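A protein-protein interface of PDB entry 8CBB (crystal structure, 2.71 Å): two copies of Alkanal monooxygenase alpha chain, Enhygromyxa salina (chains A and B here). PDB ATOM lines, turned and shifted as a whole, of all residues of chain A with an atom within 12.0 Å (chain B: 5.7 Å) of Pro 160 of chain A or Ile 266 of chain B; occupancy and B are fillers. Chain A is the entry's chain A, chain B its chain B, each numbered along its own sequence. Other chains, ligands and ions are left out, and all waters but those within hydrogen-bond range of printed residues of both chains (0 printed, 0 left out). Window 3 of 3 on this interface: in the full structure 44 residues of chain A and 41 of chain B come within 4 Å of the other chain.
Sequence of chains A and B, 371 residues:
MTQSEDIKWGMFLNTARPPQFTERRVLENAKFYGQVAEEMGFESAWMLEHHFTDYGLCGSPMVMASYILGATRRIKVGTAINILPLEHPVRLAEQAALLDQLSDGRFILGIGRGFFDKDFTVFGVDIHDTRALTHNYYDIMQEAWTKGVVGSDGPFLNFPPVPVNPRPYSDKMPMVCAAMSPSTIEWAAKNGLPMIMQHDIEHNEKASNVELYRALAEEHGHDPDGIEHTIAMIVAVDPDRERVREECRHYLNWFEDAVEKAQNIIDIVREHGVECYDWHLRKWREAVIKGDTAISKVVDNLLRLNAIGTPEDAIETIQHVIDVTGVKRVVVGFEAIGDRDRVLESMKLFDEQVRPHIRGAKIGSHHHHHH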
ATOM      1  N   HIS A  88      -0.226  24.481 -11.814  1.00  0.00           N
ATOM      2  CA  HIS A  88      -0.323  23.056 -12.078  1.00  0.00           C
ATOM      3  C   HIS A  88      -1.790  22.637 -12.053  1.00  0.00           C
ATOM      4  O   HIS A  88      -2.532  23.021 -11.151  1.00  0.00           O
ATOM      5  CB  HIS A  88       0.508  22.265 -11.059  1.00  0.00           C
ATOM      6  CG  HIS A  88       0.940  20.906 -11.522  1.00  0.00           C
ATOM      7  ND1 HIS A  88       0.087  19.835 -11.649  1.00  0.00           N
ATOM      8  CD2 HIS A  88       2.179  20.472 -11.891  1.00  0.00           C
ATOM      9  CE1 HIS A  88       0.774  18.780 -12.083  1.00  0.00           C
ATOM     10  NE2 HIS A  88       2.077  19.154 -12.241  1.00  0.00           N
ATOM     11  N   PRO A  89      -2.254  21.845 -13.046  1.00  0.00           N
ATOM     12  CA  PRO A  89      -3.671  21.496 -13.155  1.00  0.00           C
ATOM     13  C   PRO A  89      -4.127  20.508 -12.084  1.00  0.00           C
ATOM     14  O   PRO A  89      -5.317  20.403 -11.799  1.00  0.00           O
ATOM     15  CB  PRO A  89      -3.772  20.872 -14.555  1.00  0.00           C
ATOM     16  CG  PRO A  89      -2.395  20.292 -14.801  1.00  0.00           C
ATOM     17  CD  PRO A  89      -1.442  21.252 -14.118  1.00  0.00           C
ATOM     18  N   VAL A  90      -3.166  19.787 -11.497  1.00  0.00           N
ATOM     19  CA  VAL A  90      -3.463  18.819 -10.454  1.00  0.00           C
ATOM     20  C   VAL A  90      -3.701  19.568  -9.145  1.00  0.00           C
ATOM     21  O   VAL A  90      -4.442  19.101  -8.283  1.00  0.00           O
ATOM     22  CB  VAL A  90      -2.331  17.782 -10.308  1.00  0.00           C
ATOM     23  CG1 VAL A  90      -2.630  16.775  -9.207  1.00  0.00           C
ATOM     24  CG2 VAL A  90      -2.045  17.070 -11.621  1.00  0.00           C
ATOM     25  N   ARG A  91      -3.062  20.735  -9.014  1.00  0.00           N
ATOM     26  CA  ARG A  91      -3.148  21.531  -7.802  1.00  0.00           C
ATOM     27  C   ARG A  91      -4.486  22.266  -7.780  1.00  0.00           C
ATOM     28  O   ARG A  91      -5.136  22.342  -6.739  1.00  0.00           O
ATOM     29  CB  ARG A  91      -1.966  22.503  -7.722  1.00  0.00           C
ATOM     30  CG  ARG A  91      -1.914  23.320  -6.438  1.00  0.00           C
ATOM     31  CD  ARG A  91      -0.559  23.266  -5.754  1.00  0.00           C
ATOM     32  NE  ARG A  91       0.551  23.377  -6.691  1.00  0.00           N
ATOM     33  CZ  ARG A  91       0.825  24.459  -7.415  1.00  0.00           C
ATOM     34  NH1 ARG A  91       1.719  24.395  -8.388  1.00  0.00           N
ATOM     35  NH2 ARG A  91       0.206  25.600  -7.163  1.00  0.00           N
ATOM     36  N   GLU A  94      -7.363  19.929  -7.139  1.00  0.00           N
ATOM     37  CA  GLU A  94      -7.502  19.761  -5.703  1.00  0.00           C
ATOM     38  C   GLU A  94      -8.260  20.953  -5.122  1.00  0.00           C
ATOM     39  O   GLU A  94      -9.133  20.782  -4.275  1.00  0.00           O
ATOM     40  CB  GLU A  94      -6.126  19.605  -5.053  1.00  0.00           C
ATOM     41  CG  GLU A  94      -5.567  18.196  -5.147  1.00  0.00           C
ATOM     42  CD  GLU A  94      -4.110  18.055  -4.741  1.00  0.00           C
ATOM     43  OE1 GLU A  94      -3.637  16.904  -4.631  1.00  0.00           O
ATOM     44  OE2 GLU A  94      -3.449  19.094  -4.538  1.00  0.00           O
ATOM     45  N   ILE A 140      -6.858  17.480 -17.988  1.00  0.00           N
ATOM     46  CA  ILE A 140      -6.290  16.778 -16.850  1.00  0.00           C
ATOM     47  C   ILE A 140      -7.202  16.971 -15.640  1.00  0.00           C
ATOM     48  O   ILE A 140      -7.494  16.020 -14.919  1.00  0.00           O
ATOM     49  CB  ILE A 140      -4.854  17.265 -16.575  1.00  0.00           C
ATOM     50  CG1 ILE A 140      -3.885  16.801 -17.666  1.00  0.00           C
ATOM     51  CG2 ILE A 140      -4.389  16.841 -15.191  1.00  0.00           C
ATOM     52  CD1 ILE A 140      -2.605  17.602 -17.734  1.00  0.00           C
ATOM     53  N   GLU A 143     -10.404  15.078 -16.091  1.00  0.00           N
ATOM     54  CA  GLU A 143     -10.165  13.653 -15.936  1.00  0.00           C
ATOM     55  C   GLU A 143     -10.037  13.320 -14.451  1.00  0.00           C
ATOM     56  O   GLU A 143     -10.447  12.248 -14.013  1.00  0.00           O
ATOM     57  CB  GLU A 143      -8.905  13.244 -16.700  1.00  0.00           C
ATOM     58  CG  GLU A 143      -8.636  11.750 -16.677  1.00  0.00           C
ATOM     59  CD  GLU A 143      -7.657  11.272 -17.736  1.00  0.00           C
ATOM     60  OE1 GLU A 143      -7.378  10.056 -17.773  1.00  0.00           O
ATOM     61  OE2 GLU A 143      -7.177  12.116 -18.522  1.00  0.00           O
ATOM     62  N   ALA A 144      -9.464  14.256 -13.689  1.00  0.00           N
ATOM     63  CA  ALA A 144      -9.248  14.070 -12.264  1.00  0.00           C
ATOM     64  C   ALA A 144     -10.589  14.051 -11.534  1.00  0.00           C
ATOM     65  O   ALA A 144     -10.745  13.358 -10.532  1.00  0.00           O
ATOM     66  CB  ALA A 144      -8.348  15.161 -11.736  1.00  0.00           C
ATOM     67  N   GLY A 148     -11.295  10.265 -11.115  1.00  0.00           N
ATOM     68  CA  GLY A 148     -10.765  10.266  -9.761  1.00  0.00           C
ATOM     69  C   GLY A 148      -9.279   9.921  -9.733  1.00  0.00           C
ATOM     70  O   GLY A 148      -8.661   9.899  -8.671  1.00  0.00           O
ATOM     71  N   VAL A 149      -8.724   9.648 -10.919  1.00  0.00           N
ATOM     72  CA  VAL A 149      -7.306   9.365 -11.071  1.00  0.00           C
ATOM     73  C   VAL A 149      -6.844   9.941 -12.408  1.00  0.00           C
ATOM     74  O   VAL A 149      -7.598   9.953 -13.378  1.00  0.00           O
ATOM     75  CB  VAL A 149      -7.023   7.852 -10.976  1.00  0.00           C
ATOM     76  CG1 VAL A 149      -7.781   7.066 -12.034  1.00  0.00           C
ATOM     77  CG2 VAL A 149      -5.535   7.546 -11.052  1.00  0.00           C
ATOM     78  N   VAL A 150      -5.599  10.426 -12.440  1.00  0.00           N
ATOM     79  CA  VAL A 150      -5.081  11.124 -13.604  1.00  0.00           C
ATOM     80  C   VAL A 150      -3.557  11.037 -13.598  1.00  0.00           C
ATOM     81  O   VAL A 150      -2.913  11.315 -12.589  1.00  0.00           O
ATOM     82  CB  VAL A 150      -5.560  12.589 -13.642  1.00  0.00           C
ATOM     83  CG1 VAL A 150      -5.105  13.367 -12.417  1.00  0.00           C
ATOM     84  CG2 VAL A 150      -5.122  13.291 -14.917  1.00  0.00           C
ATOM     85  N   GLY A 151      -2.993  10.640 -14.744  1.00  0.00           N
ATOM     86  CA  GLY A 151      -1.580  10.829 -15.021  1.00  0.00           C
ATOM     87  C   GLY A 151      -1.368  11.661 -16.282  1.00  0.00           C
ATOM     88  O   GLY A 151      -2.323  12.177 -16.858  1.00  0.00           O
ATOM     89  N   SER A 152      -0.103  11.781 -16.699  1.00  0.00           N
ATOM     90  CA  SER A 152       0.246  12.515 -17.903  1.00  0.00           C
ATOM     91  C   SER A 152       1.652  12.132 -18.351  1.00  0.00           C
ATOM     92  O   SER A 152       2.634  12.521 -17.723  1.00  0.00           O
ATOM     93  CB  SER A 152       0.127  14.001 -17.682  1.00  0.00           C
ATOM     94  OG  SER A 152       0.521  14.720 -18.840  1.00  0.00           O
ATOM     95  N   ASP A 153       1.732  11.361 -19.441  1.00  0.00           N
ATOM     96  CA  ASP A 153       2.893  11.384 -20.316  1.00  0.00           C
ATOM     97  C   ASP A 153       2.611  12.335 -21.476  1.00  0.00           C
ATOM     98  O   ASP A 153       2.889  12.017 -22.631  1.00  0.00           O
ATOM     99  CB  ASP A 153       3.259   9.975 -20.796  1.00  0.00           C
ATOM    100  CG  ASP A 153       2.080   9.168 -21.314  1.00  0.00           C
ATOM    101  OD1 ASP A 153       1.570   8.321 -20.552  1.00  0.00           O
ATOM    102  OD2 ASP A 153       1.686   9.386 -22.477  1.00  0.00           O
ATOM    103  N   GLY A 154       2.057  13.507 -21.144  1.00  0.00           N
ATOM    104  CA  GLY A 154       1.521  14.418 -22.140  1.00  0.00           C
ATOM    105  C   GLY A 154       2.616  15.296 -22.735  1.00  0.00           C
ATOM    106  O   GLY A 154       3.800  15.059 -22.503  1.00  0.00           O
ATOM    107  N   PHE A 156       3.419  18.360 -22.105  1.00  0.00           N
ATOM    108  CA  PHE A 156       3.857  19.439 -21.233  1.00  0.00           C
ATOM    109  C   PHE A 156       4.278  18.873 -19.880  1.00  0.00           C
ATOM    110  O   PHE A 156       5.371  19.161 -19.394  1.00  0.00           O
ATOM    111  CB  PHE A 156       2.748  20.482 -21.072  1.00  0.00           C
ATOM    112  CG  PHE A 156       2.267  21.087 -22.367  1.00  0.00           C
ATOM    113  CD1 PHE A 156       3.140  21.770 -23.199  1.00  0.00           C
ATOM    114  CD2 PHE A 156       0.942  20.967 -22.757  1.00  0.00           C
ATOM    115  CE1 PHE A 156       2.697  22.321 -24.392  1.00  0.00           C
ATOM    116  CE2 PHE A 156       0.501  21.519 -23.950  1.00  0.00           C
ATOM    117  CZ  PHE A 156       1.379  22.195 -24.765  1.00  0.00           C
ATOM    118  N   LEU A 157       3.396  18.072 -19.277  1.00  0.00           N
ATOM    119  CA  LEU A 157       3.642  17.506 -17.961  1.00  0.00           C
ATOM    120  C   LEU A 157       3.812  15.994 -18.080  1.00  0.00           C
ATOM    121  O   LEU A 157       3.147  15.350 -18.888  1.00  0.00           O
ATOM    122  CB  LEU A 157       2.472  17.864 -17.039  1.00  0.00           C
ATOM    123  CG  LEU A 157       2.175  19.358 -16.908  1.00  0.00           C
ATOM    124  CD1 LEU A 157       0.962  19.593 -16.019  1.00  0.00           C
ATOM    125  CD2 LEU A 157       3.384  20.107 -16.369  1.00  0.00           C
ATOM    126  N   ASN A 158       4.716  15.445 -17.260  1.00  0.00           N
ATOM    127  CA  ASN A 158       4.964  14.013 -17.224  1.00  0.00           C
ATOM    128  C   ASN A 158       4.939  13.539 -15.774  1.00  0.00           C
ATOM    129  O   ASN A 158       5.882  13.778 -15.022  1.00  0.00           O
ATOM    130  CB  ASN A 158       6.293  13.652 -17.896  1.00  0.00           C
ATOM    131  CG  ASN A 158       6.328  14.014 -19.366  1.00  0.00           C
ATOM    132  OD1 ASN A 158       6.652  15.144 -19.725  1.00  0.00           O
ATOM    133  ND2 ASN A 158       6.000  13.060 -20.222  1.00  0.00           N
ATOM    134  N   PHE A 159       3.848  12.867 -15.392  1.00  0.00           N
ATOM    135  CA  PHE A 159       3.742  12.267 -14.073  1.00  0.00           C
ATOM    136  C   PHE A 159       2.848  11.033 -14.143  1.00  0.00           C
ATOM    137  O   PHE A 159       1.932  10.964 -14.961  1.00  0.00           O
ATOM    138  CB  PHE A 159       3.216  13.287 -13.058  1.00  0.00           C
ATOM    139  CG  PHE A 159       1.906  13.939 -13.427  1.00  0.00           C
ATOM    140  CD1 PHE A 159       0.700  13.311 -13.159  1.00  0.00           C
ATOM    141  CD2 PHE A 159       1.880  15.183 -14.037  1.00  0.00           C
ATOM    142  CE1 PHE A 159      -0.502  13.912 -13.495  1.00  0.00           C
ATOM    143  CE2 PHE A 159       0.677  15.782 -14.375  1.00  0.00           C
ATOM    144  CZ  PHE A 159      -0.512  15.146 -14.103  1.00  0.00           C
ATOM    145  N   PRO A 160       3.088  10.017 -13.284  1.00  0.00           N
ATOM    146  CA  PRO A 160       2.305   8.784 -13.311  1.00  0.00           C
ATOM    147  C   PRO A 160       0.877   9.003 -12.822  1.00  0.00           C
ATOM    148  O   PRO A 160       0.592   9.987 -12.144  1.00  0.00           O
ATOM    149  CB  PRO A 160       3.078   7.846 -12.371  1.00  0.00           C
ATOM    150  CG  PRO A 160       3.794   8.780 -11.417  1.00  0.00           C
ATOM    151  CD  PRO A 160       4.124  10.009 -12.240  1.00  0.00           C
ATOM    152  N   PRO A 161      -0.064   8.092 -13.156  1.00  0.00           N
ATOM    153  CA  PRO A 161      -1.432   8.171 -12.643  1.00  0.00           C
ATOM    154  C   PRO A 161      -1.480   8.152 -11.117  1.00  0.00           C
ATOM    155  O   PRO A 161      -0.883   7.282 -10.484  1.00  0.00           O
ATOM    156  CB  PRO A 161      -2.119   6.924 -13.224  1.00  0.00           C
ATOM    157  CG  PRO A 161      -1.273   6.548 -14.426  1.00  0.00           C
ATOM    158  CD  PRO A 161       0.140   6.946 -14.055  1.00  0.00           C
ATOM    159  N   VAL A 162      -2.200   9.121 -10.541  1.00  0.00           N
ATOM    160  CA  VAL A 162      -2.428   9.171  -9.106  1.00  0.00           C
ATOM    161  C   VAL A 162      -3.858   9.641  -8.851  1.00  0.00           C
ATOM    162  O   VAL A 162      -4.389  10.462  -9.596  1.00  0.00           O
ATOM    163  CB  VAL A 162      -1.410  10.089  -8.402  1.00  0.00           C
ATOM    164  CG1 VAL A 162      -0.028   9.457  -8.339  1.00  0.00           C
ATOM    165  CG2 VAL A 162      -1.344  11.463  -9.052  1.00  0.00           C
ATOM    166  N   PRO A 163      -4.522   9.141  -7.784  1.00  0.00           N
ATOM    167  CA  PRO A 163      -5.831   9.655  -7.386  1.00  0.00           C
ATOM    168  C   PRO A 163      -5.744  11.098  -6.899  1.00  0.00           C
ATOM    169  O   PRO A 163      -4.801  11.469  -6.204  1.00  0.00           O
ATOM    170  CB  PRO A 163      -6.274   8.704  -6.263  1.00  0.00           C
ATOM    171  CG  PRO A 163      -4.979   8.140  -5.716  1.00  0.00           C
ATOM    172  CD  PRO A 163      -4.044   8.063  -6.906  1.00  0.00           C
ATOM    173  N   VAL A 164      -6.738  11.904  -7.285  1.00  0.00           N
ATOM    174  CA  VAL A 164      -6.832  13.286  -6.846  1.00  0.00           C
ATOM    175  C   VAL A 164      -8.078  13.432  -5.979  1.00  0.00           C
ATOM    176  O   VAL A 164      -9.183  13.114  -6.417  1.00  0.00           O
ATOM    177  CB  VAL A 164      -6.867  14.252  -8.046  1.00  0.00           C
ATOM    178  CG1 VAL A 164      -7.192  15.675  -7.619  1.00  0.00           C
ATOM    179  CG2 VAL A 164      -5.569  14.213  -8.839  1.00  0.00           C
ATOM    180  N   ASN A 165      -7.881  13.914  -4.748  1.00  0.00           N
ATOM    181  CA  ASN A 165      -8.964  14.060  -3.790  1.00  0.00           C
ATOM    182  C   ASN A 165      -9.119  15.536  -3.430  1.00  0.00           C
ATOM    183  O   ASN A 165      -8.195  16.324  -3.623  1.00  0.00           O
ATOM    184  CB  ASN A 165      -8.727  13.202  -2.545  1.00  0.00           C
ATOM    185  CG  ASN A 165      -8.374  11.767  -2.876  1.00  0.00           C
ATOM    186  OD1 ASN A 165      -8.980  11.160  -3.757  1.00  0.00           O
ATOM    187  ND2 ASN A 165      -7.392  11.218  -2.179  1.00  0.00           N
ATOM    188  N   ASP B 117       7.510  11.188  -1.547  1.00  0.00           N
ATOM    189  CA  ASP B 117       8.209  11.172  -2.822  1.00  0.00           C
ATOM    190  C   ASP B 117       7.191  11.299  -3.953  1.00  0.00           C
ATOM    191  O   ASP B 117       7.509  11.802  -5.028  1.00  0.00           O
ATOM    192  CB  ASP B 117       9.047   9.899  -2.974  1.00  0.00           C
ATOM    193  CG  ASP B 117      10.208  10.037  -3.946  1.00  0.00           C
ATOM    194  OD1 ASP B 117      11.215  10.669  -3.570  1.00  0.00           O
ATOM    195  OD2 ASP B 117      10.095   9.508  -5.072  1.00  0.00           O
ATOM    196  N   LYS B 118       5.965  10.833  -3.691  1.00  0.00           N
ATOM    197  CA  LYS B 118       4.871  10.946  -4.641  1.00  0.00           C
ATOM    198  C   LYS B 118       4.631  12.416  -4.979  1.00  0.00           C
ATOM    199  O   LYS B 118       4.369  12.757  -6.131  1.00  0.00           O
ATOM    200  CB  LYS B 118       3.605  10.305  -4.065  1.00  0.00           C
ATOM    201  CG  LYS B 118       3.059  10.969  -2.807  1.00  0.00           C
ATOM    202  CD  LYS B 118       1.835  10.282  -2.242  1.00  0.00           C
ATOM    203  CE  LYS B 118       1.467  10.773  -0.857  1.00  0.00           C
ATOM    204  NZ  LYS B 118       1.315  12.247  -0.823  1.00  0.00           N
ATOM    205  N   THR B 121       7.297  13.888  -7.339  1.00  0.00           N
ATOM    206  CA  THR B 121       7.237  13.243  -8.640  1.00  0.00           C
ATOM    207  C   THR B 121       6.157  13.906  -9.492  1.00  0.00           C
ATOM    208  O   THR B 121       6.379  14.191 -10.667  1.00  0.00           O
ATOM    209  CB  THR B 121       6.979  11.738  -8.494  1.00  0.00           C
ATOM    210  OG1 THR B 121       8.136  11.144  -7.903  1.00  0.00           O
ATOM    211  CG2 THR B 121       6.676  11.060  -9.813  1.00  0.00           C
ATOM    212  N   VAL B 122       4.989  14.142  -8.885  1.00  0.00           N
ATOM    213  CA  VAL B 122       3.792  14.503  -9.626  1.00  0.00           C
ATOM    214  C   VAL B 122       3.885  15.970 -10.040  1.00  0.00           C
ATOM    215  O   VAL B 122       3.513  16.329 -11.154  1.00  0.00           O
ATOM    216  CB  VAL B 122       2.519  14.235  -8.799  1.00  0.00           C
ATOM    217  CG1 VAL B 122       1.296  14.906  -9.406  1.00  0.00           C
ATOM    218  CG2 VAL B 122       2.272  12.746  -8.611  1.00  0.00           C
ATOM    219  N   ASN B 264       3.802   4.722  -1.247  1.00  0.00           N
ATOM    220  CA  ASN B 264       3.783   3.556  -2.115  1.00  0.00           C
ATOM    221  C   ASN B 264       2.751   3.744  -3.226  1.00  0.00           C
ATOM    222  O   ASN B 264       2.515   2.827  -4.010  1.00  0.00           O
ATOM    223  CB  ASN B 264       3.486   2.271  -1.335  1.00  0.00           C
ATOM    224  CG  ASN B 264       4.677   1.753  -0.555  1.00  0.00           C
ATOM    225  OD1 ASN B 264       5.817   1.868  -1.001  1.00  0.00           O
ATOM    226  ND2 ASN B 264       4.423   1.178   0.610  1.00  0.00           N
ATOM    227  N   ILE B 265       2.141   4.933  -3.285  1.00  0.00           N
ATOM    228  CA  ILE B 265       0.868   5.109  -3.969  1.00  0.00           C
ATOM    229  C   ILE B 265       1.071   4.909  -5.469  1.00  0.00           C
ATOM    230  O   ILE B 265       0.221   4.324  -6.137  1.00  0.00           O
ATOM    231  CB  ILE B 265       0.250   6.488  -3.658  1.00  0.00           C
ATOM    232  CG1 ILE B 265      -1.104   6.673  -4.349  1.00  0.00           C
ATOM    233  CG2 ILE B 265       1.215   7.609  -4.013  1.00  0.00           C
ATOM    234  CD1 ILE B 265      -2.115   5.594  -4.030  1.00  0.00           C
ATOM    235  N   ILE B 266       2.202   5.403  -5.985  1.00  0.00           N
ATOM    236  CA  ILE B 266       2.442   5.450  -7.419  1.00  0.00           C
ATOM    237  C   ILE B 266       2.576   4.025  -7.949  1.00  0.00           C
ATOM    238  O   ILE B 266       2.188   3.738  -9.080  1.00  0.00           O
ATOM    239  CB  ILE B 266       3.688   6.301  -7.739  1.00  0.00           C
ATOM    240  CG1 ILE B 266       3.387   7.800  -7.650  1.00  0.00           C
ATOM    241  CG2 ILE B 266       4.270   5.923  -9.093  1.00  0.00           C
ATOM    242  CD1 ILE B 266       4.622   8.667  -7.531  1.00  0.00           C
ATOM    243  N   ASP B 267       3.127   3.139  -7.111  1.00  0.00           N
ATOM    244  CA  ASP B 267       3.407   1.769  -7.505  1.00  0.00           C
ATOM    245  C   ASP B 267       2.109   0.963  -7.489  1.00  0.00           C
ATOM    246  O   ASP B 267       2.000  -0.057  -8.166  1.00  0.00           O
ATOM    247  CB  ASP B 267       4.463   1.143  -6.589  1.00  0.00           C
ATOM    248  CG  ASP B 267       5.659   0.577  -7.332  1.00  0.00           C
ATOM    249  OD1 ASP B 267       5.443  -0.217  -8.270  1.00  0.00           O
ATOM    250  OD2 ASP B 267       6.798   0.934  -6.967  1.00  0.00           O
ATOM    251  N   ILE B 268       1.132   1.438  -6.708  1.00  0.00           N
ATOM    252  CA  ILE B 268      -0.099   0.702  -6.466  1.00  0.00           C
ATOM    253  C   ILE B 268      -1.086   0.985  -7.597  1.00  0.00           C
ATOM    254  O   ILE B 268      -1.936   0.153  -7.905  1.00  0.00           O
ATOM    255  CB  ILE B 268      -0.690   1.064  -5.088  1.00  0.00           C
ATOM    256  CG1 ILE B 268       0.158   0.506  -3.942  1.00  0.00           C
ATOM    257  CG2 ILE B 268      -2.140   0.613  -4.985  1.00  0.00           C
ATOM    258  CD1 ILE B 268      -0.163   1.104  -2.591  1.00  0.00           C
ATOM    259  N   VAL B 269      -0.961   2.171  -8.207  1.00  0.00           N
ATOM    260  CA  VAL B 269      -1.864   2.592  -9.266  1.00  0.00           C
ATOM    261  C   VAL B 269      -1.429   1.934 -10.574  1.00  0.00           C
ATOM    262  O   VAL B 269      -2.221   1.830 -11.517  1.00  0.00           O
ATOM    263  CB  VAL B 269      -1.903   4.127  -9.398  1.00  0.00           C
ATOM    264  CG1 VAL B 269      -2.935   4.580 -10.420  1.00  0.00           C
ATOM    265  CG2 VAL B 269      -2.144   4.803  -8.057  1.00  0.00           C
ATOM    266  N   ARG B 270      -0.160   1.496 -10.615  1.00  0.00           N
ATOM    267  CA  ARG B 270       0.374   0.797 -11.772  1.00  0.00           C
ATOM    268  C   ARG B 270       0.061  -0.693 -11.653  1.00  0.00           C
ATOM    269  O   ARG B 270      -0.064  -1.387 -12.660  1.00  0.00           O
ATOM    270  CB  ARG B 270       1.883   1.038 -11.885  1.00  0.00           C
ATOM    271  CG  ARG B 270       2.500   0.539 -13.184  1.00  0.00           C
ATOM    272  CD  ARG B 270       3.947   0.119 -13.006  1.00  0.00           C
ATOM    273  NE  ARG B 270       4.085  -0.984 -12.061  1.00  0.00           N
ATOM    274  CZ  ARG B 270       5.244  -1.443 -11.595  1.00  0.00           C
ATOM    275  NH1 ARG B 270       5.264  -2.442 -10.722  1.00  0.00           N
ATOM    276  NH2 ARG B 270       6.381  -0.902 -12.006  1.00  0.00           N
ATOM    277  N   GLU B 271      -0.061  -1.170 -10.408  1.00  0.00           N
ATOM    278  CA  GLU B 271      -0.369  -2.567 -10.141  1.00  0.00           C
ATOM    279  C   GLU B 271      -1.864  -2.801 -10.345  1.00  0.00           C
ATOM    280  O   GLU B 271      -2.262  -3.569 -11.219  1.00  0.00           O
ATOM    281  CB  GLU B 271       0.059  -2.947  -8.722  1.00  0.00           C
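The backbone carbonyl oxygen (O) of Val 150 of chain A sits at hydrogen-bond distance from the backbone NH (N) of Val 162 of chain A (3.1 Å).
The backbone carbonyl oxygen of Ser 152 of chain A sits at hydrogen-bond distance from the backbone NH of Phe 159 of chain A, 2.7 Å away.
A ring nitrogen (ND1) of His 88 of chain A lies close to the backbone NH of Val 90 of chain A, 3.3 Å away.
The side-chain hydroxyl (OG1) of Thr 121 of chain B lies within hydrogen-bond range of the backbone carbonyl oxygen (O) of Asp 117 of chain B (3.0 Å).
NE2 of His 88 of chain A lies within hydrogen-bond range of O of Val 122 of chain B, at 3.4 Å.
Of the 25 printed residues of chain A, 7 touch a printed residue of chain B.
Of the 12 printed residues of chain B, 4 touch a printed residue of chain A.
Hydrophobic or aromatic side chains of chain B that line the printed part of chain A: Val 122, Ile 266 and Val 269.
Among the printed residues, 9 pairs touch across the chains.
Among the printed residues, no Asp or Glu carboxylate lies within 4 Å of a Lys or Arg side-chain nitrogen of the other chain.
No position is printed for both chains.
Among the printed residues, pairs that only touch across the chains: Val 149 of chain A with Val 269 of chain B (3.99 Å), Phe 159 of chain A with Val 122 of chain B (3.5 Å), Pro 160 of chain A with Thr 121 of chain B (3.7 Å), Pro 160 of chain A with Ile 266 of chain B (3.7 Å), Pro 161 of chain A with Val 269 of chain B (3.4 Å), Val 162 of chain A with Val 122 of chain B (3.9 Å), Val 162 of chain A with Ile 266 of chain B (3.9 Å) and Pro 163 of chain A with Val 269 of chain B (3.9 Å).
Of chain B, only Thr 121 and Ile 266 come within 4 Å of Pro 160 of chain A.
Ile 266 of chain B touches just these residues of chain A: Pro 160 and Val 162.
Val 122 of chain B touches just these residues of chain A: His 88 (3.4 Å), Phe 159 (3.5 Å) and Val 162 (3.9 Å).
No residue of chain A comes within 4 Å of Ile 265 of chain B.
No residue of chain A comes within 4 Å of Asp 267 of chain B.
No residue of chain A comes within 4 Å of Ile 268 of chain B.
No residue of chain A comes within 4 Å of Arg 270 of chain B.
Printed residues of chain B within 4 Å of Pro 163 of chain A: Val 269.
Printed residues of chain B within 4 Å of Val 149 of chain A: Val 269.
Of the printed residues of chain B, Val 162 of chain A touches Val 122 (3.9 Å) and Ile 266 (3.9 Å).
Printed residues of chain B within 4 Å of His 88 of chain A: Val 122.
Of the printed residues of chain B, Phe 159 of chain A touches Val 122 (3.5 Å).
Glu 94 of chain A touches none of the printed residues of chain B.
Gly 154 of chain A touches none of the printed residues of chain B.
The nearest residue of chain B that does not touch Pro 160 of chain A is Val 122 of chain B (4.8 Å).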
